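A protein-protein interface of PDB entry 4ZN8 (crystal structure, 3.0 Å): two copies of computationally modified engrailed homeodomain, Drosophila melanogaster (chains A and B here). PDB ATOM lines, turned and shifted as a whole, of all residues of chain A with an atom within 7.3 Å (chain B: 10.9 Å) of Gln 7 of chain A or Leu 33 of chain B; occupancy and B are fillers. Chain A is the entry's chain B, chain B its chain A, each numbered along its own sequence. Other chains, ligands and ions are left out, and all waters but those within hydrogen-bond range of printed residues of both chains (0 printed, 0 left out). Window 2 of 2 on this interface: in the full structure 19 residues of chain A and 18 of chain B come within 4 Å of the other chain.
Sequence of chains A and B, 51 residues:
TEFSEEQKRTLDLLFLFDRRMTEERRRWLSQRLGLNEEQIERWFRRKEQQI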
ATOM      1  N   GLU A   2       9.312  29.102 -20.539  1.00  0.00           N
ATOM      2  CA  GLU A   2      10.583  28.391 -20.468  1.00  0.00           C
ATOM      3  C   GLU A   2      10.749  27.699 -19.116  1.00  0.00           C
ATOM      4  O   GLU A   2      11.419  26.670 -19.009  1.00  0.00           O
ATOM      5  CB  GLU A   2      11.749  29.354 -20.719  1.00  0.00           C
ATOM      6  CG  GLU A   2      13.127  28.708 -20.661  1.00  0.00           C
ATOM      7  CD  GLU A   2      14.250  29.693 -20.938  1.00  0.00           C
ATOM      8  OE1 GLU A   2      13.965  30.797 -21.445  1.00  0.00           O
ATOM      9  OE2 GLU A   2      15.418  29.360 -20.645  1.00  0.00           O
ATOM     10  N   PHE A   3      10.120  28.260 -18.089  1.00  0.00           N
ATOM     11  CA  PHE A   3      10.290  27.768 -16.727  1.00  0.00           C
ATOM     12  C   PHE A   3       9.068  26.997 -16.234  1.00  0.00           C
ATOM     13  O   PHE A   3       8.541  26.127 -16.930  1.00  0.00           O
ATOM     14  CB  PHE A   3      10.586  28.937 -15.782  1.00  0.00           C
ATOM     15  CG  PHE A   3      11.670  29.854 -16.276  1.00  0.00           C
ATOM     16  CD1 PHE A   3      11.355  31.017 -16.960  1.00  0.00           C
ATOM     17  CD2 PHE A   3      13.004  29.547 -16.066  1.00  0.00           C
ATOM     18  CE1 PHE A   3      12.352  31.860 -17.419  1.00  0.00           C
ATOM     19  CE2 PHE A   3      14.004  30.385 -16.522  1.00  0.00           C
ATOM     20  CZ  PHE A   3      13.678  31.542 -17.199  1.00  0.00           C
ATOM     21  N   SER A   4       8.633  27.323 -15.022  1.00  0.00           N
ATOM     22  CA  SER A   4       7.472  26.696 -14.404  1.00  0.00           C
ATOM     23  C   SER A   4       6.887  27.661 -13.385  1.00  0.00           C
ATOM     24  O   SER A   4       7.459  28.723 -13.142  1.00  0.00           O
ATOM     25  CB  SER A   4       7.852  25.373 -13.735  1.00  0.00           C
ATOM     26  OG  SER A   4       6.752  24.808 -13.041  1.00  0.00           O
ATOM     27  N   GLU A   5       5.753  27.296 -12.792  1.00  0.00           N
ATOM     28  CA  GLU A   5       5.148  28.135 -11.764  1.00  0.00           C
ATOM     29  C   GLU A   5       5.664  27.799 -10.354  1.00  0.00           C
ATOM     30  O   GLU A   5       5.739  28.687  -9.515  1.00  0.00           O
ATOM     31  CB  GLU A   5       3.618  28.055 -11.822  1.00  0.00           C
ATOM     32  CG  GLU A   5       3.030  26.671 -11.724  1.00  0.00           C
ATOM     33  CD  GLU A   5       1.522  26.712 -11.602  1.00  0.00           C
ATOM     34  OE1 GLU A   5       1.028  27.406 -10.685  1.00  0.00           O
ATOM     35  OE2 GLU A   5       0.835  26.028 -12.389  1.00  0.00           O
ATOM     36  N   GLU A   6       6.047  26.547 -10.093  1.00  0.00           N
ATOM     37  CA  GLU A   6       6.744  26.229  -8.836  1.00  0.00           C
ATOM     38  C   GLU A   6       8.261  26.223  -9.013  1.00  0.00           C
ATOM     39  O   GLU A   6       8.974  25.494  -8.320  1.00  0.00           O
ATOM     40  CB  GLU A   6       6.322  24.872  -8.265  1.00  0.00           C
ATOM     41  CG  GLU A   6       6.068  23.810  -9.305  1.00  0.00           C
ATOM     42  CD  GLU A   6       4.680  23.897  -9.904  1.00  0.00           C
ATOM     43  OE1 GLU A   6       3.971  24.883  -9.610  1.00  0.00           O
ATOM     44  OE2 GLU A   6       4.304  22.967 -10.649  1.00  0.00           O
ATOM     45  N   GLN A   7       8.748  27.028  -9.948  1.00  0.00           N
ATOM     46  CA  GLN A   7      10.182  27.210 -10.127  1.00  0.00           C
ATOM     47  C   GLN A   7      10.468  28.696 -10.248  1.00  0.00           C
ATOM     48  O   GLN A   7      11.577  29.153  -9.978  1.00  0.00           O
ATOM     49  CB  GLN A   7      10.694  26.455 -11.358  1.00  0.00           C
ATOM     50  CG  GLN A   7      10.619  24.941 -11.242  1.00  0.00           C
ATOM     51  CD  GLN A   7      11.236  24.240 -12.433  1.00  0.00           C
ATOM     52  OE1 GLN A   7      11.483  24.857 -13.469  1.00  0.00           O
ATOM     53  NE2 GLN A   7      11.498  22.946 -12.290  1.00  0.00           N
ATOM     54  N   LYS A   8       9.444  29.445 -10.642  1.00  0.00           N
ATOM     55  CA  LYS A   8       9.559  30.887 -10.795  1.00  0.00           C
ATOM     56  C   LYS A   8       9.402  31.570  -9.442  1.00  0.00           C
ATOM     57  O   LYS A   8      10.056  32.581  -9.169  1.00  0.00           O
ATOM     58  CB  LYS A   8       8.522  31.407 -11.795  1.00  0.00           C
ATOM     59  CG  LYS A   8       8.010  32.810 -11.515  1.00  0.00           C
ATOM     60  CD  LYS A   8       6.618  33.021 -12.092  1.00  0.00           C
ATOM     61  CE  LYS A   8       5.543  32.652 -11.086  1.00  0.00           C
ATOM     62  NZ  LYS A   8       5.597  33.532  -9.887  1.00  0.00           N
ATOM     63  N   ARG A   9       8.541  31.011  -8.595  1.00  0.00           N
ATOM     64  CA  ARG A   9       8.400  31.507  -7.234  1.00  0.00           C
ATOM     65  C   ARG A   9       9.735  31.416  -6.500  1.00  0.00           C
ATOM     66  O   ARG A   9      10.179  32.381  -5.880  1.00  0.00           O
ATOM     67  CB  ARG A   9       7.341  30.719  -6.470  1.00  0.00           C
ATOM     68  CG  ARG A   9       6.002  30.536  -7.173  1.00  0.00           C
ATOM     69  CD  ARG A   9       5.138  29.690  -6.270  1.00  0.00           C
ATOM     70  NE  ARG A   9       6.034  28.896  -5.434  1.00  0.00           N
ATOM     71  CZ  ARG A   9       5.667  27.881  -4.666  1.00  0.00           C
ATOM     72  NH1 ARG A   9       4.393  27.517  -4.598  1.00  0.00           N
ATOM     73  NH2 ARG A   9       6.581  27.238  -3.958  1.00  0.00           N
ATOM     74  N   THR A  10      10.357  30.242  -6.567  1.00  0.00           N
ATOM     75  CA  THR A  10      11.662  29.997  -5.959  1.00  0.00           C
ATOM     76  C   THR A  10      12.699  31.011  -6.443  1.00  0.00           C
ATOM     77  O   THR A  10      13.544  31.473  -5.673  1.00  0.00           O
ATOM     78  CB  THR A  10      12.154  28.567  -6.271  1.00  0.00           C
ATOM     79  OG1 THR A  10      11.211  27.617  -5.758  1.00  0.00           O
ATOM     80  CG2 THR A  10      13.516  28.307  -5.641  1.00  0.00           C
ATOM     81  N   LEU A  11      12.618  31.364  -7.722  1.00  0.00           N
ATOM     82  CA  LEU A  11      13.500  32.370  -8.299  1.00  0.00           C
ATOM     83  C   LEU A  11      13.078  33.779  -7.883  1.00  0.00           C
ATOM     84  O   LEU A  11      13.919  34.658  -7.704  1.00  0.00           O
ATOM     85  CB  LEU A  11      13.518  32.251  -9.824  1.00  0.00           C
ATOM     86  CG  LEU A  11      14.164  30.981 -10.380  1.00  0.00           C
ATOM     87  CD1 LEU A  11      13.855  30.819 -11.860  1.00  0.00           C
ATOM     88  CD2 LEU A  11      15.666  30.999 -10.144  1.00  0.00           C
ATOM     89  N   ASP A  12      11.772  33.986  -7.733  1.00  0.00           N
ATOM     90  CA  ASP A  12      11.248  35.275  -7.288  1.00  0.00           C
ATOM     91  C   ASP A  12      11.625  35.555  -5.840  1.00  0.00           C
ATOM     92  O   ASP A  12      11.996  36.675  -5.489  1.00  0.00           O
ATOM     93  CB  ASP A  12       9.726  35.328  -7.443  1.00  0.00           C
ATOM     94  CG  ASP A  12       9.294  35.656  -8.856  1.00  0.00           C
ATOM     95  OD1 ASP A  12       9.996  36.441  -9.526  1.00  0.00           O
ATOM     96  OD2 ASP A  12       8.246  35.137  -9.295  1.00  0.00           O
ATOM     97  N   LEU A  14      14.200  34.323  -3.966  1.00  0.00           N
ATOM     98  CA  LEU A  14      15.623  34.592  -3.796  1.00  0.00           C
ATOM     99  C   LEU A  14      16.037  35.911  -4.440  1.00  0.00           C
ATOM    100  O   LEU A  14      17.064  36.485  -4.080  1.00  0.00           O
ATOM    101  CB  LEU A  14      16.456  33.444  -4.371  1.00  0.00           C
ATOM    102  CG  LEU A  14      16.386  32.120  -3.608  1.00  0.00           C
ATOM    103  CD1 LEU A  14      17.342  31.104  -4.213  1.00  0.00           C
ATOM    104  CD2 LEU A  14      16.694  32.335  -2.134  1.00  0.00           C
ATOM    105  N   GLU B  24      27.554  29.894  -6.690  1.00  0.00           N
ATOM    106  CA  GLU B  24      27.093  28.691  -6.011  1.00  0.00           C
ATOM    107  C   GLU B  24      25.581  28.669  -5.824  1.00  0.00           C
ATOM    108  O   GLU B  24      24.978  27.598  -5.768  1.00  0.00           O
ATOM    109  CB  GLU B  24      27.792  28.552  -4.657  1.00  0.00           C
ATOM    110  CG  GLU B  24      29.309  28.473  -4.755  1.00  0.00           C
ATOM    111  CD  GLU B  24      29.786  27.253  -5.523  1.00  0.00           C
ATOM    112  OE1 GLU B  24      29.061  26.235  -5.547  1.00  0.00           O
ATOM    113  OE2 GLU B  24      30.889  27.314  -6.107  1.00  0.00           O
ATOM    114  N   ARG B  25      24.968  29.845  -5.720  1.00  0.00           N
ATOM    115  CA  ARG B  25      23.514  29.923  -5.650  1.00  0.00           C
ATOM    116  C   ARG B  25      22.913  29.454  -6.965  1.00  0.00           C
ATOM    117  O   ARG B  25      21.914  28.734  -6.984  1.00  0.00           O
ATOM    118  CB  ARG B  25      23.045  31.346  -5.341  1.00  0.00           C
ATOM    119  CG  ARG B  25      21.530  31.482  -5.310  1.00  0.00           C
ATOM    120  CD  ARG B  25      21.090  32.919  -5.121  1.00  0.00           C
ATOM    121  NE  ARG B  25      21.326  33.726  -6.312  1.00  0.00           N
ATOM    122  CZ  ARG B  25      20.915  34.981  -6.454  1.00  0.00           C
ATOM    123  NH1 ARG B  25      20.240  35.570  -5.476  1.00  0.00           N
ATOM    124  NH2 ARG B  25      21.173  35.646  -7.572  1.00  0.00           N
ATOM    125  N   ARG B  26      23.535  29.872  -8.062  1.00  0.00           N
ATOM    126  CA  ARG B  26      23.092  29.490  -9.395  1.00  0.00           C
ATOM    127  C   ARG B  26      23.197  27.983  -9.591  1.00  0.00           C
ATOM    128  O   ARG B  26      22.275  27.348 -10.101  1.00  0.00           O
ATOM    129  CB  ARG B  26      23.911  30.220 -10.456  1.00  0.00           C
ATOM    130  CG  ARG B  26      23.450  29.963 -11.876  1.00  0.00           C
ATOM    131  CD  ARG B  26      24.276  30.757 -12.869  1.00  0.00           C
ATOM    132  NE  ARG B  26      25.674  30.336 -12.890  1.00  0.00           N
ATOM    133  CZ  ARG B  26      26.689  31.102 -12.504  1.00  0.00           C
ATOM    134  NH1 ARG B  26      26.464  32.335 -12.071  1.00  0.00           N
ATOM    135  NH2 ARG B  26      27.930  30.637 -12.557  1.00  0.00           N
ATOM    136  N   ARG B  27      24.329  27.421  -9.180  1.00  0.00           N
ATOM    137  CA  ARG B  27      24.534  25.979  -9.234  1.00  0.00           C
ATOM    138  C   ARG B  27      23.516  25.240  -8.376  1.00  0.00           C
ATOM    139  O   ARG B  27      22.925  24.251  -8.811  1.00  0.00           O
ATOM    140  CB  ARG B  27      25.948  25.621  -8.780  1.00  0.00           C
ATOM    141  CG  ARG B  27      26.079  24.191  -8.290  1.00  0.00           C
ATOM    142  CD  ARG B  27      27.507  23.875  -7.914  1.00  0.00           C
ATOM    143  NE  ARG B  27      28.395  24.009  -9.060  1.00  0.00           N
ATOM    144  CZ  ARG B  27      29.714  23.894  -8.995  1.00  0.00           C
ATOM    145  NH1 ARG B  27      30.300  23.642  -7.832  1.00  0.00           N
ATOM    146  NH2 ARG B  27      30.446  24.031 -10.092  1.00  0.00           N
ATOM    147  N   TRP B  28      23.316  25.728  -7.157  1.00  0.00           N
ATOM    148  CA  TRP B  28      22.374  25.117  -6.227  1.00  0.00           C
ATOM    149  C   TRP B  28      20.950  25.179  -6.773  1.00  0.00           C
ATOM    150  O   TRP B  28      20.121  24.324  -6.463  1.00  0.00           O
ATOM    151  CB  TRP B  28      22.453  25.800  -4.860  1.00  0.00           C
ATOM    152  CG  TRP B  28      21.518  25.223  -3.846  1.00  0.00           C
ATOM    153  CD1 TRP B  28      21.708  24.088  -3.113  1.00  0.00           C
ATOM    154  CD2 TRP B  28      20.250  25.750  -3.444  1.00  0.00           C
ATOM    155  NE1 TRP B  28      20.634  23.876  -2.284  1.00  0.00           N
ATOM    156  CE2 TRP B  28      19.725  24.883  -2.467  1.00  0.00           C
ATOM    157  CE3 TRP B  28      19.506  26.876  -3.820  1.00  0.00           C
ATOM    158  CZ2 TRP B  28      18.491  25.103  -1.859  1.00  0.00           C
ATOM    159  CZ3 TRP B  28      18.282  27.092  -3.213  1.00  0.00           C
ATOM    160  CH2 TRP B  28      17.786  26.210  -2.243  1.00  0.00           C
ATOM    161  N   LEU B  29      20.676  26.192  -7.589  1.00  0.00           N
ATOM    162  CA  LEU B  29      19.381  26.318  -8.245  1.00  0.00           C
ATOM    163  C   LEU B  29      19.333  25.478  -9.514  1.00  0.00           C
ATOM    164  O   LEU B  29      18.299  24.900  -9.850  1.00  0.00           O
ATOM    165  CB  LEU B  29      19.082  27.782  -8.568  1.00  0.00           C
ATOM    166  CG  LEU B  29      18.625  28.648  -7.393  1.00  0.00           C
ATOM    167  CD1 LEU B  29      18.504  30.101  -7.819  1.00  0.00           C
ATOM    168  CD2 LEU B  29      17.302  28.137  -6.843  1.00  0.00           C
ATOM    169  N   SER B  30      20.462  25.410 -10.214  1.00  0.00           N
ATOM    170  CA  SER B  30      20.571  24.601 -11.422  1.00  0.00           C
ATOM    171  C   SER B  30      20.469  23.117 -11.094  1.00  0.00           C
ATOM    172  O   SER B  30      20.205  22.293 -11.969  1.00  0.00           O
ATOM    173  CB  SER B  30      21.888  24.890 -12.148  1.00  0.00           C
ATOM    174  OG  SER B  30      22.055  24.038 -13.268  1.00  0.00           O
ATOM    175  N   GLN B  31      20.682  22.783  -9.824  1.00  0.00           N
ATOM    176  CA  GLN B  31      20.621  21.401  -9.370  1.00  0.00           C
ATOM    177  C   GLN B  31      19.417  21.165  -8.465  1.00  0.00           C
ATOM    178  O   GLN B  31      19.389  20.204  -7.696  1.00  0.00           O
ATOM    179  CB  GLN B  31      21.910  21.028  -8.636  1.00  0.00           C
ATOM    180  CG  GLN B  31      23.165  21.125  -9.489  1.00  0.00           C
ATOM    181  CD  GLN B  31      24.435  21.084  -8.662  1.00  0.00           C
ATOM    182  OE1 GLN B  31      24.391  21.124  -7.432  1.00  0.00           O
ATOM    183  NE2 GLN B  31      25.578  21.008  -9.335  1.00  0.00           N
ATOM    184  N   ARG B  32      18.423  22.044  -8.556  1.00  0.00           N
ATOM    185  CA  ARG B  32      17.222  21.912  -7.740  1.00  0.00           C
ATOM    186  C   ARG B  32      15.968  22.264  -8.535  1.00  0.00           C
ATOM    187  O   ARG B  32      14.871  21.805  -8.217  1.00  0.00           O
ATOM    188  CB  ARG B  32      17.321  22.793  -6.492  1.00  0.00           C
ATOM    189  CG  ARG B  32      16.246  22.516  -5.453  1.00  0.00           C
ATOM    190  CD  ARG B  32      16.400  23.412  -4.239  1.00  0.00           C
ATOM    191  NE  ARG B  32      15.380  23.136  -3.231  1.00  0.00           N
ATOM    192  CZ  ARG B  32      14.166  23.677  -3.228  1.00  0.00           C
ATOM    193  NH1 ARG B  32      13.814  24.530  -4.181  1.00  0.00           N
ATOM    194  NH2 ARG B  32      13.302  23.368  -2.269  1.00  0.00           N
ATOM    195  N   LEU B  33      16.135  23.077  -9.574  1.00  0.00           N
ATOM    196  CA  LEU B  33      15.015  23.454 -10.427  1.00  0.00           C
ATOM    197  C   LEU B  33      15.082  22.736 -11.772  1.00  0.00           C
ATOM    198  O   LEU B  33      14.175  22.854 -12.595  1.00  0.00           O
ATOM    199  CB  LEU B  33      14.983  24.970 -10.636  1.00  0.00           C
ATOM    200  CG  LEU B  33      14.760  25.811  -9.377  1.00  0.00           C
ATOM    201  CD1 LEU B  33      14.718  27.294  -9.717  1.00  0.00           C
ATOM    202  CD2 LEU B  33      13.484  25.384  -8.664  1.00  0.00           C
ATOM    203  N   GLY B  34      16.164  21.993 -11.987  1.00  0.00           N
ATOM    204  CA  GLY B  34      16.330  21.218 -13.203  1.00  0.00           C
ATOM    205  C   GLY B  34      16.857  22.029 -14.372  1.00  0.00           C
ATOM    206  O   GLY B  34      17.295  21.473 -15.379  1.00  0.00           O
ATOM    207  N   LEU B  35      16.811  23.349 -14.236  1.00  0.00           N
ATOM    208  CA  LEU B  35      17.277  24.252 -15.281  1.00  0.00           C
ATOM    209  C   LEU B  35      18.801  24.344 -15.246  1.00  0.00           C
ATOM    210  O   LEU B  35      19.439  23.712 -14.404  1.00  0.00           O
ATOM    211  CB  LEU B  35      16.641  25.631 -15.106  1.00  0.00           C
ATOM    212  CG  LEU B  35      15.158  25.579 -14.727  1.00  0.00           C
ATOM    213  CD1 LEU B  35      14.631  26.965 -14.393  1.00  0.00           C
ATOM    214  CD2 LEU B  35      14.331  24.939 -15.835  1.00  0.00           C
ATOM    215  N   ASN B  36      19.387  25.121 -16.150  1.00  0.00           N
ATOM    216  CA  ASN B  36      20.844  25.215 -16.211  1.00  0.00           C
ATOM    217  C   ASN B  36      21.372  26.603 -15.848  1.00  0.00           C
ATOM    218  O   ASN B  36      20.604  27.549 -15.681  1.00  0.00           O
ATOM    219  CB  ASN B  36      21.346  24.800 -17.599  1.00  0.00           C
ATOM    220  CG  ASN B  36      20.713  25.600 -18.721  1.00  0.00           C
ATOM    221  OD1 ASN B  36      20.703  26.829 -18.698  1.00  0.00           O
ATOM    222  ND2 ASN B  36      20.180  24.898 -19.716  1.00  0.00           N
ATOM    223  N   GLU B  37      22.693  26.712 -15.738  1.00  0.00           N
ATOM    224  CA  GLU B  37      23.329  27.922 -15.225  1.00  0.00           C
ATOM    225  C   GLU B  37      23.308  29.087 -16.213  1.00  0.00           C
ATOM    226  O   GLU B  37      23.714  30.197 -15.875  1.00  0.00           O
ATOM    227  CB  GLU B  37      24.771  27.623 -14.809  1.00  0.00           C
ATOM    228  CG  GLU B  37      24.886  26.654 -13.643  1.00  0.00           C
ATOM    229  CD  GLU B  37      26.197  26.795 -12.895  1.00  0.00           C
ATOM    230  OE1 GLU B  37      26.797  27.888 -12.951  1.00  0.00           O
ATOM    231  OE2 GLU B  37      26.625  25.814 -12.253  1.00  0.00           O
ATOM    232  N   GLN B  39      20.308  29.317 -17.982  1.00  0.00           N
ATOM    233  CA  GLN B  39      18.883  29.568 -17.798  1.00  0.00           C
ATOM    234  C   GLN B  39      18.658  30.392 -16.539  1.00  0.00           C
ATOM    235  O   GLN B  39      18.007  31.436 -16.572  1.00  0.00           O
ATOM    236  CB  GLN B  39      18.096  28.260 -17.700  1.00  0.00           C
ATOM    237  CG  GLN B  39      17.681  27.656 -19.029  1.00  0.00           C
ATOM    238  CD  GLN B  39      16.893  26.374 -18.852  1.00  0.00           C
ATOM    239  OE1 GLN B  39      17.425  25.364 -18.393  1.00  0.00           O
ATOM    240  NE2 GLN B  39      15.613  26.411 -19.208  1.00  0.00           N
ATOM    241  N   ILE B  40      19.204  29.902 -15.429  1.00  0.00           N
ATOM    242  CA  ILE B  40      19.066  30.558 -14.133  1.00  0.00           C
ATOM    243  C   ILE B  40      19.646  31.967 -14.156  1.00  0.00           C
ATOM    244  O   ILE B  40      19.013  32.915 -13.689  1.00  0.00           O
ATOM    245  CB  ILE B  40      19.759  29.747 -13.019  1.00  0.00           C
ATOM    246  CG1 ILE B  40      19.152  28.346 -12.919  1.00  0.00           C
ATOM    247  CG2 ILE B  40      19.649  30.469 -11.686  1.00  0.00           C
ATOM    248  CD1 ILE B  40      17.688  28.340 -12.540  1.00  0.00           C
ATOM    249  N   GLU B  41      20.848  32.103 -14.707  1.00  0.00           N
ATOM    250  CA  GLU B  41      21.513  33.399 -14.768  1.00  0.00           C
ATOM    251  C   GLU B  41      20.797  34.334 -15.736  1.00  0.00           C
ATOM    252  O   GLU B  41      20.859  35.555 -15.591  1.00  0.00           O
ATOM    253  CB  GLU B  41      22.978  33.235 -15.173  1.00  0.00           C
ATOM    254  CG  GLU B  41      23.815  34.489 -14.984  1.00  0.00           C
ATOM    255  CD  GLU B  41      25.292  34.252 -15.238  1.00  0.00           C
ATOM    256  OE1 GLU B  41      25.631  33.231 -15.874  1.00  0.00           O
ATOM    257  OE2 GLU B  41      26.112  35.084 -14.797  1.00  0.00           O
ATOM    258  N   TRP B  43      17.449  34.312 -16.146  1.00  0.00           N
ATOM    259  CA  TRP B  43      16.278  34.749 -15.395  1.00  0.00           C
ATOM    260  C   TRP B  43      16.633  35.874 -14.428  1.00  0.00           C
ATOM    261  O   TRP B  43      15.884  36.841 -14.288  1.00  0.00           O
ATOM    262  CB  TRP B  43      15.661  33.575 -14.631  1.00  0.00           C
ATOM    263  CG  TRP B  43      14.324  33.893 -14.038  1.00  0.00           C
ATOM    264  CD1 TRP B  43      13.103  33.610 -14.577  1.00  0.00           C
ATOM    265  CD2 TRP B  43      14.069  34.563 -12.797  1.00  0.00           C
ATOM    266  NE1 TRP B  43      12.104  34.057 -13.748  1.00  0.00           N
ATOM    267  CE2 TRP B  43      12.670  34.647 -12.649  1.00  0.00           C
ATOM    268  CE3 TRP B  43      14.886  35.098 -11.798  1.00  0.00           C
ATOM    269  CZ2 TRP B  43      12.073  35.244 -11.541  1.00  0.00           C
ATOM    270  CZ3 TRP B  43      14.292  35.691 -10.702  1.00  0.00           C
ATOM    271  CH2 TRP B  43      12.899  35.760 -10.582  1.00  0.00           C
ATOM    272  N   PHE B  44      17.776  35.744 -13.763  1.00  0.00           N
ATOM    273  CA  PHE B  44      18.215  36.752 -12.804  1.00  0.00           C
ATOM    274  C   PHE B  44      18.691  38.023 -13.499  1.00  0.00           C
ATOM    275  O   PHE B  44      18.641  39.107 -12.919  1.00  0.00           O
ATOM    276  CB  PHE B  44      19.325  36.197 -11.907  1.00  0.00           C
ATOM    277  CG  PHE B  44      18.815  35.406 -10.735  1.00  0.00           C
ATOM    278  CD1 PHE B  44      19.039  34.042 -10.650  1.00  0.00           C
ATOM    279  CD2 PHE B  44      18.105  36.027  -9.720  1.00  0.00           C
ATOM    280  CE1 PHE B  44      18.570  33.313  -9.574  1.00  0.00           C
ATOM    281  CE2 PHE B  44      17.633  35.304  -8.642  1.00  0.00           C
ATOM    282  CZ  PHE B  44      17.865  33.945  -8.569  1.00  0.00           C
ATOM    283  N   LYS B  47      15.103  39.820 -14.475  1.00  0.00           N
ATOM    284  CA  LYS B  47      14.430  40.485 -13.367  1.00  0.00           C
ATOM    285  C   LYS B  47      15.247  41.673 -12.862  1.00  0.00           C
ATOM    286  O   LYS B  47      14.708  42.585 -12.234  1.00  0.00           O
ATOM    287  CB  LYS B  47      14.180  39.494 -12.226  1.00  0.00           C
ATOM    288  CG  LYS B  47      13.016  39.855 -11.315  1.00  0.00           C
ATOM    289  CD  LYS B  47      11.726  39.192 -11.770  1.00  0.00           C
ATOM    290  CE  LYS B  47      10.550  39.610 -10.898  1.00  0.00           C
ATOM    291  NZ  LYS B  47       9.265  39.022 -11.370  1.00  0.00           N
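OD1 of Asp 12 of chain A lies within salt-bridge range of NZ of Lys 47 of chain B (3.3 Å). The side-chain carboxylate (OE2) of Glu 2 of chain A sits close to the side-chain amide nitrogen (NE2) of Gln 39 of chain B, 3.3 Å away. The backbone carbonyl oxygen of Leu 33 of chain B is in hydrogen-bond range of the side-chain amide nitrogen of Gln 7 of chain A (2.7 Å).
The backbone NH of Gln 39 of chain B is in hydrogen-bond range of the side-chain amide oxygen of Asn 36 of chain B, at 2.6 Å. The backbone carbonyl oxygen (O) of Leu 35 of chain B lies within hydrogen-bond range of the side-chain hydroxyl (OG) of Ser 30 of chain B, at 2.9 Å. The side-chain carboxylate of Asp 12 of chain A is in salt-bridge range of the side-chain amino group of Lys 8 of chain A, at 3.2 Å.
CD2 of Phe 3 of chain A touches CD1 of Leu 35 of chain B, 3.5 Å away. Trp 43 of chain B touches Phe 3 of chain A. Gln 7 of chain A touches Leu 35 of chain B. CD2 of Leu 29 of chain B touches CG2 of Thr 10 of chain A (3.98 Å). Leu 11 of chain A touches Leu 33 of chain B (CG to CD1, 3.8 Å). Leu 11 of chain A touches Trp 43 of chain B. CD2 of Leu 11 of chain A touches CE1 of Phe 44 of chain B, at 3.8 Å. Asp 12 of chain A touches Trp 43 of chain B. Arg 25 of chain B touches Leu 14 of chain A (NH1 to O, 3.6 Å). Leu 29 of chain B touches Leu 14 of chain A (CD1 to CD1, 3.9 Å).
Printed residues of chain B within 4 Å of Gln 7 of chain A: Leu 33 (2.7 Å) and Leu 35 (3.7 Å). Of chain A, only Gln 7 (2.7 Å) and Leu 11 (3.8 Å) come within 4 Å of Leu 33 of chain B. No residue of chain B comes within 4 Å of Ser 4 of chain A. No residue of chain B comes within 4 Å of Glu 6 of chain A. Of the printed residues of chain B, Thr 10 of chain A touches Leu 29 (3.98 Å). Of the printed residues of chain A, Lys 47 of chain B touches Asp 12 (3.3 Å). Of the printed residues of chain A, Leu 35 of chain B touches Phe 3 and Gln 7. Printed residues of chain A within 4 Å of Trp 43 of chain B: Phe 3 (3.4 Å), Leu 11 (3.2 Å) and Asp 12 (3.1 Å). The nearest residue of chain A that does not touch Leu 33 of chain B is Thr 10 of chain A (4.2 Å).
Hydrophobic or aromatic side chains of chain A within 4 Å of the printed part of chain B: Phe 3, Leu 11 and Leu 14. Among the printed residues, Asp or Glu carboxylates within 4 Å of a Lys or Arg side-chain nitrogen of the other chain: Asp 12 of chain A with Lys 47 of chain B.
No position is printed for both chains.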
